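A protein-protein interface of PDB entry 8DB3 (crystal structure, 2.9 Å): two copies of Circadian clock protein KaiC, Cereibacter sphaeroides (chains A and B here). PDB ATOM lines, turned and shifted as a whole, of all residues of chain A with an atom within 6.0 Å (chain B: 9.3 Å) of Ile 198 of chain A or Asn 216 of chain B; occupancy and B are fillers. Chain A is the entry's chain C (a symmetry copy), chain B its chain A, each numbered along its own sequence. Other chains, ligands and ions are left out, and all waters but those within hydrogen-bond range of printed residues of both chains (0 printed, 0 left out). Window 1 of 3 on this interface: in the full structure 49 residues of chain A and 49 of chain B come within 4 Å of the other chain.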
ATOM      1  N   ARG A 193     -29.034  -1.350 -23.040  1.00  0.00           N
ATOM      2  CA  ARG A 193     -28.188  -1.975 -22.033  1.00  0.00           C
ATOM      3  C   ARG A 193     -26.803  -1.345 -22.020  1.00  0.00           C
ATOM      4  O   ARG A 193     -26.182  -1.167 -23.071  1.00  0.00           O
ATOM      5  CB  ARG A 193     -28.085  -3.480 -22.281  1.00  0.00           C
ATOM      6  CG  ARG A 193     -29.232  -4.262 -21.668  1.00  0.00           C
ATOM      7  CD  ARG A 193     -28.901  -5.734 -21.545  1.00  0.00           C
ATOM      8  NE  ARG A 193     -29.425  -6.506 -22.667  1.00  0.00           N
ATOM      9  CZ  ARG A 193     -28.688  -6.972 -23.667  1.00  0.00           C
ATOM     10  NH1 ARG A 193     -27.385  -6.747 -23.732  1.00  0.00           N
ATOM     11  NH2 ARG A 193     -29.274  -7.686 -24.622  1.00  0.00           N
ATOM     12  N   VAL A 194     -26.326  -1.017 -20.821  1.00  0.00           N
ATOM     13  CA  VAL A 194     -25.027  -0.384 -20.631  1.00  0.00           C
ATOM     14  C   VAL A 194     -24.020  -1.451 -20.230  1.00  0.00           C
ATOM     15  O   VAL A 194     -24.299  -2.287 -19.361  1.00  0.00           O
ATOM     16  CB  VAL A 194     -25.094   0.724 -19.567  1.00  0.00           C
ATOM     17  CG1 VAL A 194     -23.724   1.364 -19.389  1.00  0.00           C
ATOM     18  CG2 VAL A 194     -26.130   1.765 -19.938  1.00  0.00           C
ATOM     19  N   GLU A 195     -22.845  -1.418 -20.853  1.00  0.00           N
ATOM     20  CA  GLU A 195     -21.760  -2.336 -20.530  1.00  0.00           C
ATOM     21  C   GLU A 195     -20.456  -1.561 -20.627  1.00  0.00           C
ATOM     22  O   GLU A 195     -20.116  -1.052 -21.699  1.00  0.00           O
ATOM     23  CB  GLU A 195     -21.754  -3.541 -21.473  1.00  0.00           C
ATOM     24  CG  GLU A 195     -20.765  -4.638 -21.096  1.00  0.00           C
ATOM     25  CD  GLU A 195     -20.111  -5.282 -22.312  1.00  0.00           C
ATOM     26  OE1 GLU A 195     -18.901  -5.049 -22.529  1.00  0.00           O
ATOM     27  OE2 GLU A 195     -20.805  -6.016 -23.047  1.00  0.00           O
ATOM     28  N   ASN A 196     -19.736  -1.466 -19.512  1.00  0.00           N
ATOM     29  CA  ASN A 196     -18.518  -0.663 -19.432  1.00  0.00           C
ATOM     30  C   ASN A 196     -18.791   0.772 -19.878  1.00  0.00           C
ATOM     31  O   ASN A 196     -18.123   1.320 -20.759  1.00  0.00           O
ATOM     32  CB  ASN A 196     -17.392  -1.294 -20.253  1.00  0.00           C
ATOM     33  CG  ASN A 196     -16.736  -2.463 -19.542  1.00  0.00           C
ATOM     34  OD1 ASN A 196     -17.418  -3.339 -19.006  1.00  0.00           O
ATOM     35  ND2 ASN A 196     -15.407  -2.483 -19.528  1.00  0.00           N
ATOM     36  N   GLN A 197     -19.805   1.376 -19.262  1.00  0.00           N
ATOM     37  CA  GLN A 197     -20.232   2.757 -19.458  1.00  0.00           C
ATOM     38  C   GLN A 197     -20.785   3.025 -20.854  1.00  0.00           C
ATOM     39  O   GLN A 197     -21.195   4.159 -21.130  1.00  0.00           O
ATOM     40  CB  GLN A 197     -19.099   3.759 -19.184  1.00  0.00           C
ATOM     41  CG  GLN A 197     -18.777   3.972 -17.706  1.00  0.00           C
ATOM     42  CD  GLN A 197     -17.597   4.907 -17.491  1.00  0.00           C
ATOM     43  OE1 GLN A 197     -17.104   5.527 -18.432  1.00  0.00           O
ATOM     44  NE2 GLN A 197     -17.139   5.011 -16.247  1.00  0.00           N
ATOM     45  N   ILE A 198     -20.823   2.033 -21.740  1.00  0.00           N
ATOM     46  CA  ILE A 198     -21.293   2.214 -23.109  1.00  0.00           C
ATOM     47  C   ILE A 198     -22.678   1.594 -23.232  1.00  0.00           C
ATOM     48  O   ILE A 198     -22.907   0.470 -22.769  1.00  0.00           O
ATOM     49  CB  ILE A 198     -20.328   1.586 -24.129  1.00  0.00           C
ATOM     50  CG1 ILE A 198     -18.980   2.307 -24.120  1.00  0.00           C
ATOM     51  CG2 ILE A 198     -20.941   1.627 -25.519  1.00  0.00           C
ATOM     52  CD1 ILE A 198     -19.026   3.713 -24.673  1.00  0.00           C
ATOM     53  N   SER A 199     -23.594   2.320 -23.867  1.00  0.00           N
ATOM     54  CA  SER A 199     -24.960   1.858 -24.066  1.00  0.00           C
ATOM     55  C   SER A 199     -25.134   1.306 -25.473  1.00  0.00           C
ATOM     56  O   SER A 199     -24.574   1.837 -26.438  1.00  0.00           O
ATOM     57  CB  SER A 199     -25.961   2.993 -23.832  1.00  0.00           C
ATOM     58  OG  SER A 199     -25.643   3.729 -22.666  1.00  0.00           O
ATOM     59  N   THR A 200     -25.916   0.234 -25.583  1.00  0.00           N
ATOM     60  CA  THR A 200     -26.292  -0.334 -26.868  1.00  0.00           C
ATOM     61  C   THR A 200     -27.793  -0.585 -26.865  1.00  0.00           C
ATOM     62  O   THR A 200     -28.329  -1.177 -25.919  1.00  0.00           O
ATOM     63  CB  THR A 200     -25.531  -1.630 -27.153  1.00  0.00           C
ATOM     64  OG1 THR A 200     -24.131  -1.349 -27.249  1.00  0.00           O
ATOM     65  CG2 THR A 200     -26.004  -2.243 -28.459  1.00  0.00           C
ATOM     66  N   THR A 336     -13.765   3.571 -28.597  1.00  0.00           N
ATOM     67  CA  THR A 336     -14.701   3.940 -27.538  1.00  0.00           C
ATOM     68  C   THR A 336     -15.836   4.799 -28.087  1.00  0.00           C
ATOM     69  O   THR A 336     -17.017   4.519 -27.848  1.00  0.00           O
ATOM     70  CB  THR A 336     -13.965   4.665 -26.405  1.00  0.00           C
ATOM     71  OG1 THR A 336     -14.916   5.131 -25.436  1.00  0.00           O
ATOM     72  CG2 THR A 336     -13.148   5.843 -26.928  1.00  0.00           C
ATOM     73  N   PHE A 337     -15.499   5.848 -28.831  1.00  0.00           N
ATOM     74  CA  PHE A 337     -16.505   6.611 -29.560  1.00  0.00           C
ATOM     75  C   PHE A 337     -17.028   5.773 -30.722  1.00  0.00           C
ATOM     76  O   PHE A 337     -16.302   4.967 -31.308  1.00  0.00           O
ATOM     77  CB  PHE A 337     -15.911   7.929 -30.047  1.00  0.00           C
ATOM     78  CG  PHE A 337     -16.705   8.597 -31.131  1.00  0.00           C
ATOM     79  CD1 PHE A 337     -17.980   9.082 -30.886  1.00  0.00           C
ATOM     80  CD2 PHE A 337     -16.167   8.753 -32.398  1.00  0.00           C
ATOM     81  CE1 PHE A 337     -18.703   9.702 -31.887  1.00  0.00           C
ATOM     82  CE2 PHE A 337     -16.885   9.370 -33.401  1.00  0.00           C
ATOM     83  CZ  PHE A 337     -18.151   9.852 -33.145  1.00  0.00           C
ATOM     84  N   SER A 339     -19.657   3.203 -30.553  1.00  0.00           N
ATOM     85  CA  SER A 339     -19.578   1.877 -29.950  1.00  0.00           C
ATOM     86  C   SER A 339     -19.487   0.766 -30.987  1.00  0.00           C
ATOM     87  O   SER A 339     -19.698   1.005 -32.179  1.00  0.00           O
ATOM     88  CB  SER A 339     -20.796   1.641 -29.046  1.00  0.00           C
ATOM     89  OG  SER A 339     -21.774   0.850 -29.708  1.00  0.00           O
ATOM     90  N   LEU A 340     -19.190  -0.456 -30.536  1.00  0.00           N
ATOM     91  CA  LEU A 340     -18.926  -1.554 -31.462  1.00  0.00           C
ATOM     92  C   LEU A 340     -20.055  -1.716 -32.475  1.00  0.00           C
ATOM     93  O   LEU A 340     -19.816  -1.772 -33.687  1.00  0.00           O
ATOM     94  CB  LEU A 340     -18.713  -2.854 -30.682  1.00  0.00           C
ATOM     95  CG  LEU A 340     -18.326  -4.075 -31.518  1.00  0.00           C
ATOM     96  CD1 LEU A 340     -17.278  -4.921 -30.808  1.00  0.00           C
ATOM     97  CD2 LEU A 340     -19.559  -4.909 -31.848  1.00  0.00           C
ATOM     98  N   LEU B  16     -23.464  17.285 -23.833  1.00  0.00           N
ATOM     99  CA  LEU B  16     -24.023  15.959 -24.069  1.00  0.00           C
ATOM    100  C   LEU B  16     -25.470  16.055 -24.537  1.00  0.00           C
ATOM    101  O   LEU B  16     -25.871  15.392 -25.500  1.00  0.00           O
ATOM    102  CB  LEU B  16     -23.926  15.116 -22.800  1.00  0.00           C
ATOM    103  CG  LEU B  16     -22.510  14.833 -22.299  1.00  0.00           C
ATOM    104  CD1 LEU B  16     -22.560  14.256 -20.891  1.00  0.00           C
ATOM    105  CD2 LEU B  16     -21.774  13.899 -23.251  1.00  0.00           C
ATOM    106  N   VAL B 187     -35.116  12.264 -18.567  1.00  0.00           N
ATOM    107  CA  VAL B 187     -34.757  11.545 -17.350  1.00  0.00           C
ATOM    108  C   VAL B 187     -33.244  11.395 -17.295  1.00  0.00           C
ATOM    109  O   VAL B 187     -32.628  10.890 -18.240  1.00  0.00           O
ATOM    110  CB  VAL B 187     -35.435  10.161 -17.280  1.00  0.00           C
ATOM    111  CG1 VAL B 187     -34.910   9.373 -16.084  1.00  0.00           C
ATOM    112  CG2 VAL B 187     -36.945  10.310 -17.205  1.00  0.00           C
ATOM    113  N   ILE B 188     -32.651  11.820 -16.183  1.00  0.00           N
ATOM    114  CA  ILE B 188     -31.216  11.717 -15.957  1.00  0.00           C
ATOM    115  C   ILE B 188     -31.003  10.934 -14.670  1.00  0.00           C
ATOM    116  O   ILE B 188     -31.441  11.368 -13.597  1.00  0.00           O
ATOM    117  CB  ILE B 188     -30.552  13.099 -15.865  1.00  0.00           C
ATOM    118  CG1 ILE B 188     -30.779  13.882 -17.157  1.00  0.00           C
ATOM    119  CG2 ILE B 188     -29.069  12.952 -15.581  1.00  0.00           C
ATOM    120  CD1 ILE B 188     -31.656  15.098 -16.978  1.00  0.00           C
ATOM    121  N   LEU B 189     -30.324   9.795 -14.773  1.00  0.00           N
ATOM    122  CA  LEU B 189     -30.010   8.966 -13.617  1.00  0.00           C
ATOM    123  C   LEU B 189     -28.583   9.257 -13.174  1.00  0.00           C
ATOM    124  O   LEU B 189     -27.639   9.071 -13.948  1.00  0.00           O
ATOM    125  CB  LEU B 189     -30.168   7.481 -13.937  1.00  0.00           C
ATOM    126  CG  LEU B 189     -29.722   6.532 -12.823  1.00  0.00           C
ATOM    127  CD1 LEU B 189     -30.545   6.756 -11.563  1.00  0.00           C
ATOM    128  CD2 LEU B 189     -29.818   5.082 -13.270  1.00  0.00           C
ATOM    129  N   ARG B 193     -21.395   4.797  -7.725  1.00  0.00           N
ATOM    130  CA  ARG B 193     -21.181   3.356  -7.770  1.00  0.00           C
ATOM    131  C   ARG B 193     -19.782   3.007  -7.284  1.00  0.00           C
ATOM    132  O   ARG B 193     -18.802   3.631  -7.702  1.00  0.00           O
ATOM    133  CB  ARG B 193     -21.379   2.852  -9.201  1.00  0.00           C
ATOM    134  CG  ARG B 193     -22.081   1.523  -9.307  1.00  0.00           C
ATOM    135  CD  ARG B 193     -21.931   0.958 -10.708  1.00  0.00           C
ATOM    136  NE  ARG B 193     -22.634   1.777 -11.687  1.00  0.00           N
ATOM    137  CZ  ARG B 193     -22.172   2.071 -12.896  1.00  0.00           C
ATOM    138  NH1 ARG B 193     -21.005   1.617 -13.319  1.00  0.00           N
ATOM    139  NH2 ARG B 193     -22.906   2.838 -13.699  1.00  0.00           N
ATOM    140  N   ARG B 202     -21.566   8.714 -11.854  1.00  0.00           N
ATOM    141  CA  ARG B 202     -21.913   8.660 -13.263  1.00  0.00           C
ATOM    142  C   ARG B 202     -23.296   9.257 -13.481  1.00  0.00           C
ATOM    143  O   ARG B 202     -24.178   9.167 -12.619  1.00  0.00           O
ATOM    144  CB  ARG B 202     -21.875   7.224 -13.797  1.00  0.00           C
ATOM    145  CG  ARG B 202     -20.470   6.660 -13.917  1.00  0.00           C
ATOM    146  CD  ARG B 202     -20.497   5.210 -14.370  1.00  0.00           C
ATOM    147  NE  ARG B 202     -19.268   4.509 -14.018  1.00  0.00           N
ATOM    148  CZ  ARG B 202     -18.919   4.179 -12.782  1.00  0.00           C
ATOM    149  NH1 ARG B 202     -19.691   4.466 -11.748  1.00  0.00           N
ATOM    150  NH2 ARG B 202     -17.766   3.549 -12.580  1.00  0.00           N
ATOM    151  N   LEU B 203     -23.461   9.878 -14.647  1.00  0.00           N
ATOM    152  CA  LEU B 203     -24.709  10.478 -15.096  1.00  0.00           C
ATOM    153  C   LEU B 203     -25.102   9.815 -16.408  1.00  0.00           C
ATOM    154  O   LEU B 203     -24.259   9.621 -17.287  1.00  0.00           O
ATOM    155  CB  LEU B 203     -24.542  11.990 -15.281  1.00  0.00           C
ATOM    156  CG  LEU B 203     -25.578  12.769 -16.089  1.00  0.00           C
ATOM    157  CD1 LEU B 203     -25.618  14.227 -15.619  1.00  0.00           C
ATOM    158  CD2 LEU B 203     -25.309  12.718 -17.585  1.00  0.00           C
ATOM    159  N   ARG B 204     -26.380   9.457 -16.536  1.00  0.00           N
ATOM    160  CA  ARG B 204     -26.850   8.838 -17.769  1.00  0.00           C
ATOM    161  C   ARG B 204     -28.170   9.460 -18.191  1.00  0.00           C
ATOM    162  O   ARG B 204     -29.078   9.610 -17.370  1.00  0.00           O
ATOM    163  CB  ARG B 204     -27.028   7.323 -17.603  1.00  0.00           C
ATOM    164  CG  ARG B 204     -27.126   6.587 -18.926  1.00  0.00           C
ATOM    165  CD  ARG B 204     -28.106   5.433 -18.861  1.00  0.00           C
ATOM    166  NE  ARG B 204     -28.129   4.689 -20.114  1.00  0.00           N
ATOM    167  CZ  ARG B 204     -28.700   3.503 -20.272  1.00  0.00           C
ATOM    168  NH1 ARG B 204     -29.305   2.890 -19.269  1.00  0.00           N
ATOM    169  NH2 ARG B 204     -28.659   2.916 -21.465  1.00  0.00           N
ATOM    170  N   ILE B 205     -28.277   9.816 -19.468  1.00  0.00           N
ATOM    171  CA  ILE B 205     -29.512  10.327 -20.029  1.00  0.00           C
ATOM    172  C   ILE B 205     -30.352   9.116 -20.430  1.00  0.00           C
ATOM    173  O   ILE B 205     -30.175   8.558 -21.519  1.00  0.00           O
ATOM    174  CB  ILE B 205     -29.261  11.269 -21.216  1.00  0.00           C
ATOM    175  CG1 ILE B 205     -28.205  12.318 -20.855  1.00  0.00           C
ATOM    176  CG2 ILE B 205     -30.566  11.947 -21.631  1.00  0.00           C
ATOM    177  CD1 ILE B 205     -28.669  13.354 -19.855  1.00  0.00           C
ATOM    178  N   VAL B 206     -31.241   8.689 -19.535  1.00  0.00           N
ATOM    179  CA  VAL B 206     -32.052   7.514 -19.823  1.00  0.00           C
ATOM    180  C   VAL B 206     -33.030   7.814 -20.950  1.00  0.00           C
ATOM    181  O   VAL B 206     -33.201   7.012 -21.877  1.00  0.00           O
ATOM    182  CB  VAL B 206     -32.786   7.047 -18.554  1.00  0.00           C
ATOM    183  CG1 VAL B 206     -33.571   5.769 -18.831  1.00  0.00           C
ATOM    184  CG2 VAL B 206     -31.798   6.836 -17.421  1.00  0.00           C
ATOM    185  N   HIS B 213     -28.783  12.780 -28.337  1.00  0.00           N
ATOM    186  CA  HIS B 213     -28.043  13.103 -27.126  1.00  0.00           C
ATOM    187  C   HIS B 213     -27.144  11.928 -26.783  1.00  0.00           C
ATOM    188  O   HIS B 213     -27.304  10.821 -27.305  1.00  0.00           O
ATOM    189  CB  HIS B 213     -28.980  13.402 -25.962  1.00  0.00           C
ATOM    190  CG  HIS B 213     -29.794  12.221 -25.540  1.00  0.00           C
ATOM    191  ND1 HIS B 213     -29.382  11.340 -24.564  1.00  0.00           N
ATOM    192  CD2 HIS B 213     -30.988  11.761 -25.982  1.00  0.00           C
ATOM    193  CE1 HIS B 213     -30.292  10.395 -24.415  1.00  0.00           C
ATOM    194  NE2 HIS B 213     -31.280  10.631 -25.258  1.00  0.00           N
ATOM    195  N   GLY B 214     -26.201  12.185 -25.880  1.00  0.00           N
ATOM    196  CA  GLY B 214     -25.276  11.152 -25.453  1.00  0.00           C
ATOM    197  C   GLY B 214     -25.978  10.115 -24.602  1.00  0.00           C
ATOM    198  O   GLY B 214     -26.512  10.440 -23.527  1.00  0.00           O
ATOM    199  N   THR B 215     -25.974   8.863 -25.051  1.00  0.00           N
ATOM    200  CA  THR B 215     -26.703   7.802 -24.372  1.00  0.00           C
ATOM    201  C   THR B 215     -25.856   7.026 -23.372  1.00  0.00           C
ATOM    202  O   THR B 215     -26.413   6.258 -22.579  1.00  0.00           O
ATOM    203  CB  THR B 215     -27.282   6.821 -25.402  1.00  0.00           C
ATOM    204  OG1 THR B 215     -26.227   6.323 -26.236  1.00  0.00           O
ATOM    205  CG2 THR B 215     -28.326   7.510 -26.267  1.00  0.00           C
ATOM    206  N   ASN B 216     -24.538   7.208 -23.382  1.00  0.00           N
ATOM    207  CA  ASN B 216     -23.659   6.442 -22.518  1.00  0.00           C
ATOM    208  C   ASN B 216     -23.703   6.976 -21.088  1.00  0.00           C
ATOM    209  O   ASN B 216     -24.374   7.967 -20.781  1.00  0.00           O
ATOM    210  CB  ASN B 216     -22.227   6.478 -23.052  1.00  0.00           C
ATOM    211  CG  ASN B 216     -22.067   5.713 -24.348  1.00  0.00           C
ATOM    212  OD1 ASN B 216     -22.855   4.819 -24.658  1.00  0.00           O
ATOM    213  ND2 ASN B 216     -21.040   6.061 -25.114  1.00  0.00           N
ATOM    214  N   GLU B 217     -22.978   6.298 -20.197  1.00  0.00           N
ATOM    215  CA  GLU B 217     -22.740   6.784 -18.847  1.00  0.00           C
ATOM    216  C   GLU B 217     -21.524   7.702 -18.865  1.00  0.00           C
ATOM    217  O   GLU B 217     -20.464   7.326 -19.376  1.00  0.00           O
ATOM    218  CB  GLU B 217     -22.505   5.626 -17.881  1.00  0.00           C
ATOM    219  CG  GLU B 217     -23.747   4.829 -17.542  1.00  0.00           C
ATOM    220  CD  GLU B 217     -23.442   3.657 -16.633  1.00  0.00           C
ATOM    221  OE1 GLU B 217     -22.266   3.235 -16.580  1.00  0.00           O
ATOM    222  OE2 GLU B 217     -24.375   3.161 -15.964  1.00  0.00           O
ATOM    223  N   TYR B 218     -21.676   8.897 -18.307  1.00  0.00           N
ATOM    224  CA  TYR B 218     -20.633   9.913 -18.314  1.00  0.00           C
ATOM    225  C   TYR B 218     -20.209  10.184 -16.880  1.00  0.00           C
ATOM    226  O   TYR B 218     -21.044  10.612 -16.065  1.00  0.00           O
ATOM    227  CB  TYR B 218     -21.147  11.186 -18.986  1.00  0.00           C
ATOM    228  CG  TYR B 218     -21.536  10.962 -20.430  1.00  0.00           C
ATOM    229  CD1 TYR B 218     -20.568  10.693 -21.387  1.00  0.00           C
ATOM    230  CD2 TYR B 218     -22.867  10.997 -20.834  1.00  0.00           C
ATOM    231  CE1 TYR B 218     -20.903  10.477 -22.703  1.00  0.00           C
ATOM    232  CE2 TYR B 218     -23.213  10.783 -22.160  1.00  0.00           C
ATOM    233  CZ  TYR B 218     -22.223  10.520 -23.088  1.00  0.00           C
ATOM    234  OH  TYR B 218     -22.526  10.300 -24.412  1.00  0.00           O
ATOM    235  N   PRO B 219     -18.962   9.914 -16.505  1.00  0.00           N
ATOM    236  CA  PRO B 219     -18.539  10.220 -15.133  1.00  0.00           C
ATOM    237  C   PRO B 219     -18.473  11.721 -14.911  1.00  0.00           C
ATOM    238  O   PRO B 219     -18.072  12.485 -15.792  1.00  0.00           O
ATOM    239  CB  PRO B 219     -17.152   9.573 -15.026  1.00  0.00           C
ATOM    240  CG  PRO B 219     -17.105   8.571 -16.134  1.00  0.00           C
ATOM    241  CD  PRO B 219     -17.927   9.164 -17.241  1.00  0.00           C
ATOM    242  N   VAL B 229     -18.676  17.966 -15.502  1.00  0.00           N
ATOM    243  CA  VAL B 229     -18.529  16.835 -16.411  1.00  0.00           C
ATOM    244  C   VAL B 229     -17.465  17.193 -17.440  1.00  0.00           C
ATOM    245  O   VAL B 229     -17.417  18.330 -17.925  1.00  0.00           O
ATOM    246  CB  VAL B 229     -19.861  16.479 -17.105  1.00  0.00           C
ATOM    247  CG1 VAL B 229     -19.773  15.107 -17.764  1.00  0.00           C
ATOM    248  CG2 VAL B 229     -21.014  16.516 -16.106  1.00  0.00           C
ATOM    249  N   GLU B 341     -11.154   8.010 -14.976  1.00  0.00           N
ATOM    250  CA  GLU B 341     -11.756   9.182 -15.600  1.00  0.00           C
ATOM    251  C   GLU B 341     -11.508  10.433 -14.766  1.00  0.00           C
ATOM    252  O   GLU B 341     -11.274  11.515 -15.315  1.00  0.00           O
ATOM    253  CB  GLU B 341     -13.250   8.937 -15.810  1.00  0.00           C
ATOM    254  CG  GLU B 341     -13.548   7.919 -16.910  1.00  0.00           C
ATOM    255  CD  GLU B 341     -13.898   6.542 -16.368  1.00  0.00           C
ATOM    256  OE1 GLU B 341     -13.078   5.965 -15.623  1.00  0.00           O
ATOM    257  OE2 GLU B 341     -14.993   6.035 -16.694  1.00  0.00           O
ATOM    258  N   LEU B 374      -9.990  -2.230 -20.689  1.00  0.00           N
ATOM    259  CA  LEU B 374     -10.731  -1.335 -21.571  1.00  0.00           C
ATOM    260  C   LEU B 374     -10.770   0.083 -21.016  1.00  0.00           C
ATOM    261  O   LEU B 374     -10.672   1.059 -21.771  1.00  0.00           O
ATOM    262  CB  LEU B 374     -12.150  -1.867 -21.783  1.00  0.00           C
ATOM    263  N   SER B 378      -9.275   3.314 -23.016  1.00  0.00           N
ATOM    264  CA  SER B 378     -10.046   4.513 -23.322  1.00  0.00           C
ATOM    265  C   SER B 378      -9.378   5.758 -22.750  1.00  0.00           C
ATOM    266  O   SER B 378      -9.289   6.790 -23.426  1.00  0.00           O
ATOM    267  CB  SER B 378     -11.470   4.373 -22.783  1.00  0.00           C
ATOM    268  OG  SER B 378     -12.309   5.395 -23.292  1.00  0.00           O
ATOM    269  N   ARG B 382      -7.928   8.883 -24.939  1.00  0.00           N
ATOM    270  CA  ARG B 382      -8.433  10.234 -24.727  1.00  0.00           C
ATOM    271  C   ARG B 382      -7.304  11.212 -24.435  1.00  0.00           C
ATOM    272  O   ARG B 382      -7.315  12.346 -24.929  1.00  0.00           O
ATOM    273  CB  ARG B 382      -9.448  10.236 -23.588  1.00  0.00           C
ATOM    274  CG  ARG B 382     -10.865  10.504 -24.050  1.00  0.00           C
ATOM    275  CD  ARG B 382     -11.742  11.001 -22.914  1.00  0.00           C
ATOM    276  NE  ARG B 382     -12.367   9.902 -22.188  1.00  0.00           N
ATOM    277  CZ  ARG B 382     -13.180   9.004 -22.730  1.00  0.00           C
ATOM    278  NH1 ARG B 382     -13.513   9.054 -24.010  1.00  0.00           N
ATOM    279  NH2 ARG B 382     -13.667   8.028 -21.970  1.00  0.00           N
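O of Arg 204 of chain B sits at hydrogen-bond distance from N of Leu 189 of chain B (2.9 Å).
The side-chain carboxylate (OE2) of Glu 217 of chain B lies within salt-bridge range of the guanidinium group (NH2) of Arg 193 of chain B, at 2.7 Å.
NE of Arg 204 of chain B sits at hydrogen-bond distance from O of Thr 215 of chain B.
OG of Ser 378 of chain B is in hydrogen-bond range of NH2 of Arg 382 of chain B.
Of chain B, only Asn 216 (3.1 Å) comes within 4 Å of Ile 198 of chain A.
Asn 216 of chain B touches three residues of chain A.
Of chain B, only Arg 204 (3.3 Å), Thr 215 (2.6 Å) and Asn 216 (2.7 Å) come within 4 Å of Ser 199 of chain A.
Printed residues of chain A within 4 Å of Thr 215 of chain B: Ser 199.
Of the printed residues of chain B, Gln 197 of chain A touches Arg 202, Asn 216, Glu 217, Pro 219 and Glu 341.
Of the printed residues of chain A, Glu 217 of chain B touches Val 194 (3.6 Å) and Gln 197 (2.9 Å).
Printed residues of chain A within 4 Å of Arg 204 of chain B: Val 194 and Ser 199.
Of the printed residues of chain A, Arg 202 of chain B touches Gln 197.
Leu 374 of chain B touches none of the printed residues of chain A.
The nearest residue of chain A that does not touch Asn 216 of chain B is Thr 336 of chain A (5.1 Å).
Hydrophobic or aromatic side chains of chain B that line the printed part of chain A: Pro 219.
Of the 12 printed residues of chain A, 5 touch a printed residue of chain B.
Among the printed residues, 12 pairs touch across the chains.
Among the printed residues, no Asp or Glu carboxylate lies within 4 Å of a Lys or Arg side-chain nitrogen of the other chain.
Position printed for both chains: 193.
Of the 12 pairs that touch across the chains among the printed residues, none has its exchanged pair printed and touching as well.
NE of Arg 202 of chain B sits close to NE2 of Gln 197 of chain A (3.1 Å).
NH2 of Arg 204 of chain B lies within hydrogen-bond range of OG of Ser 199 of chain A (3.3 Å).
OG of Ser 199 of chain A lies within hydrogen-bond range of O of Thr 215 of chain B (2.6 Å).
OD1 of Asn 216 of chain B is in hydrogen-bond range of N of Ser 199 of chain A.
The backbone carbonyl oxygen (O) of Gln 197 of chain A is in hydrogen-bond range of the backbone NH (N) of Glu 217 of chain B (2.9 Å).
OE2 of Glu 341 of chain B lies within hydrogen-bond range of NE2 of Gln 197 of chain A, 2.4 Å away.
The side-chain hydroxyl (OG) of Ser 378 of chain B is in hydrogen-bond range of the side-chain hydroxyl (OG1) of Thr 336 of chain A, at 3.4 Å.
Among the printed residues, pairs that only touch across the chains: Val 194 of chain A with Arg 204 of chain B, Val 194 of chain A with Glu 217 of chain B, Gln 197 of chain A with Asn 216 of chain B, Gln 197 of chain A with Pro 219 of chain B and Ile 198 of chain A with Asn 216 of chain B.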
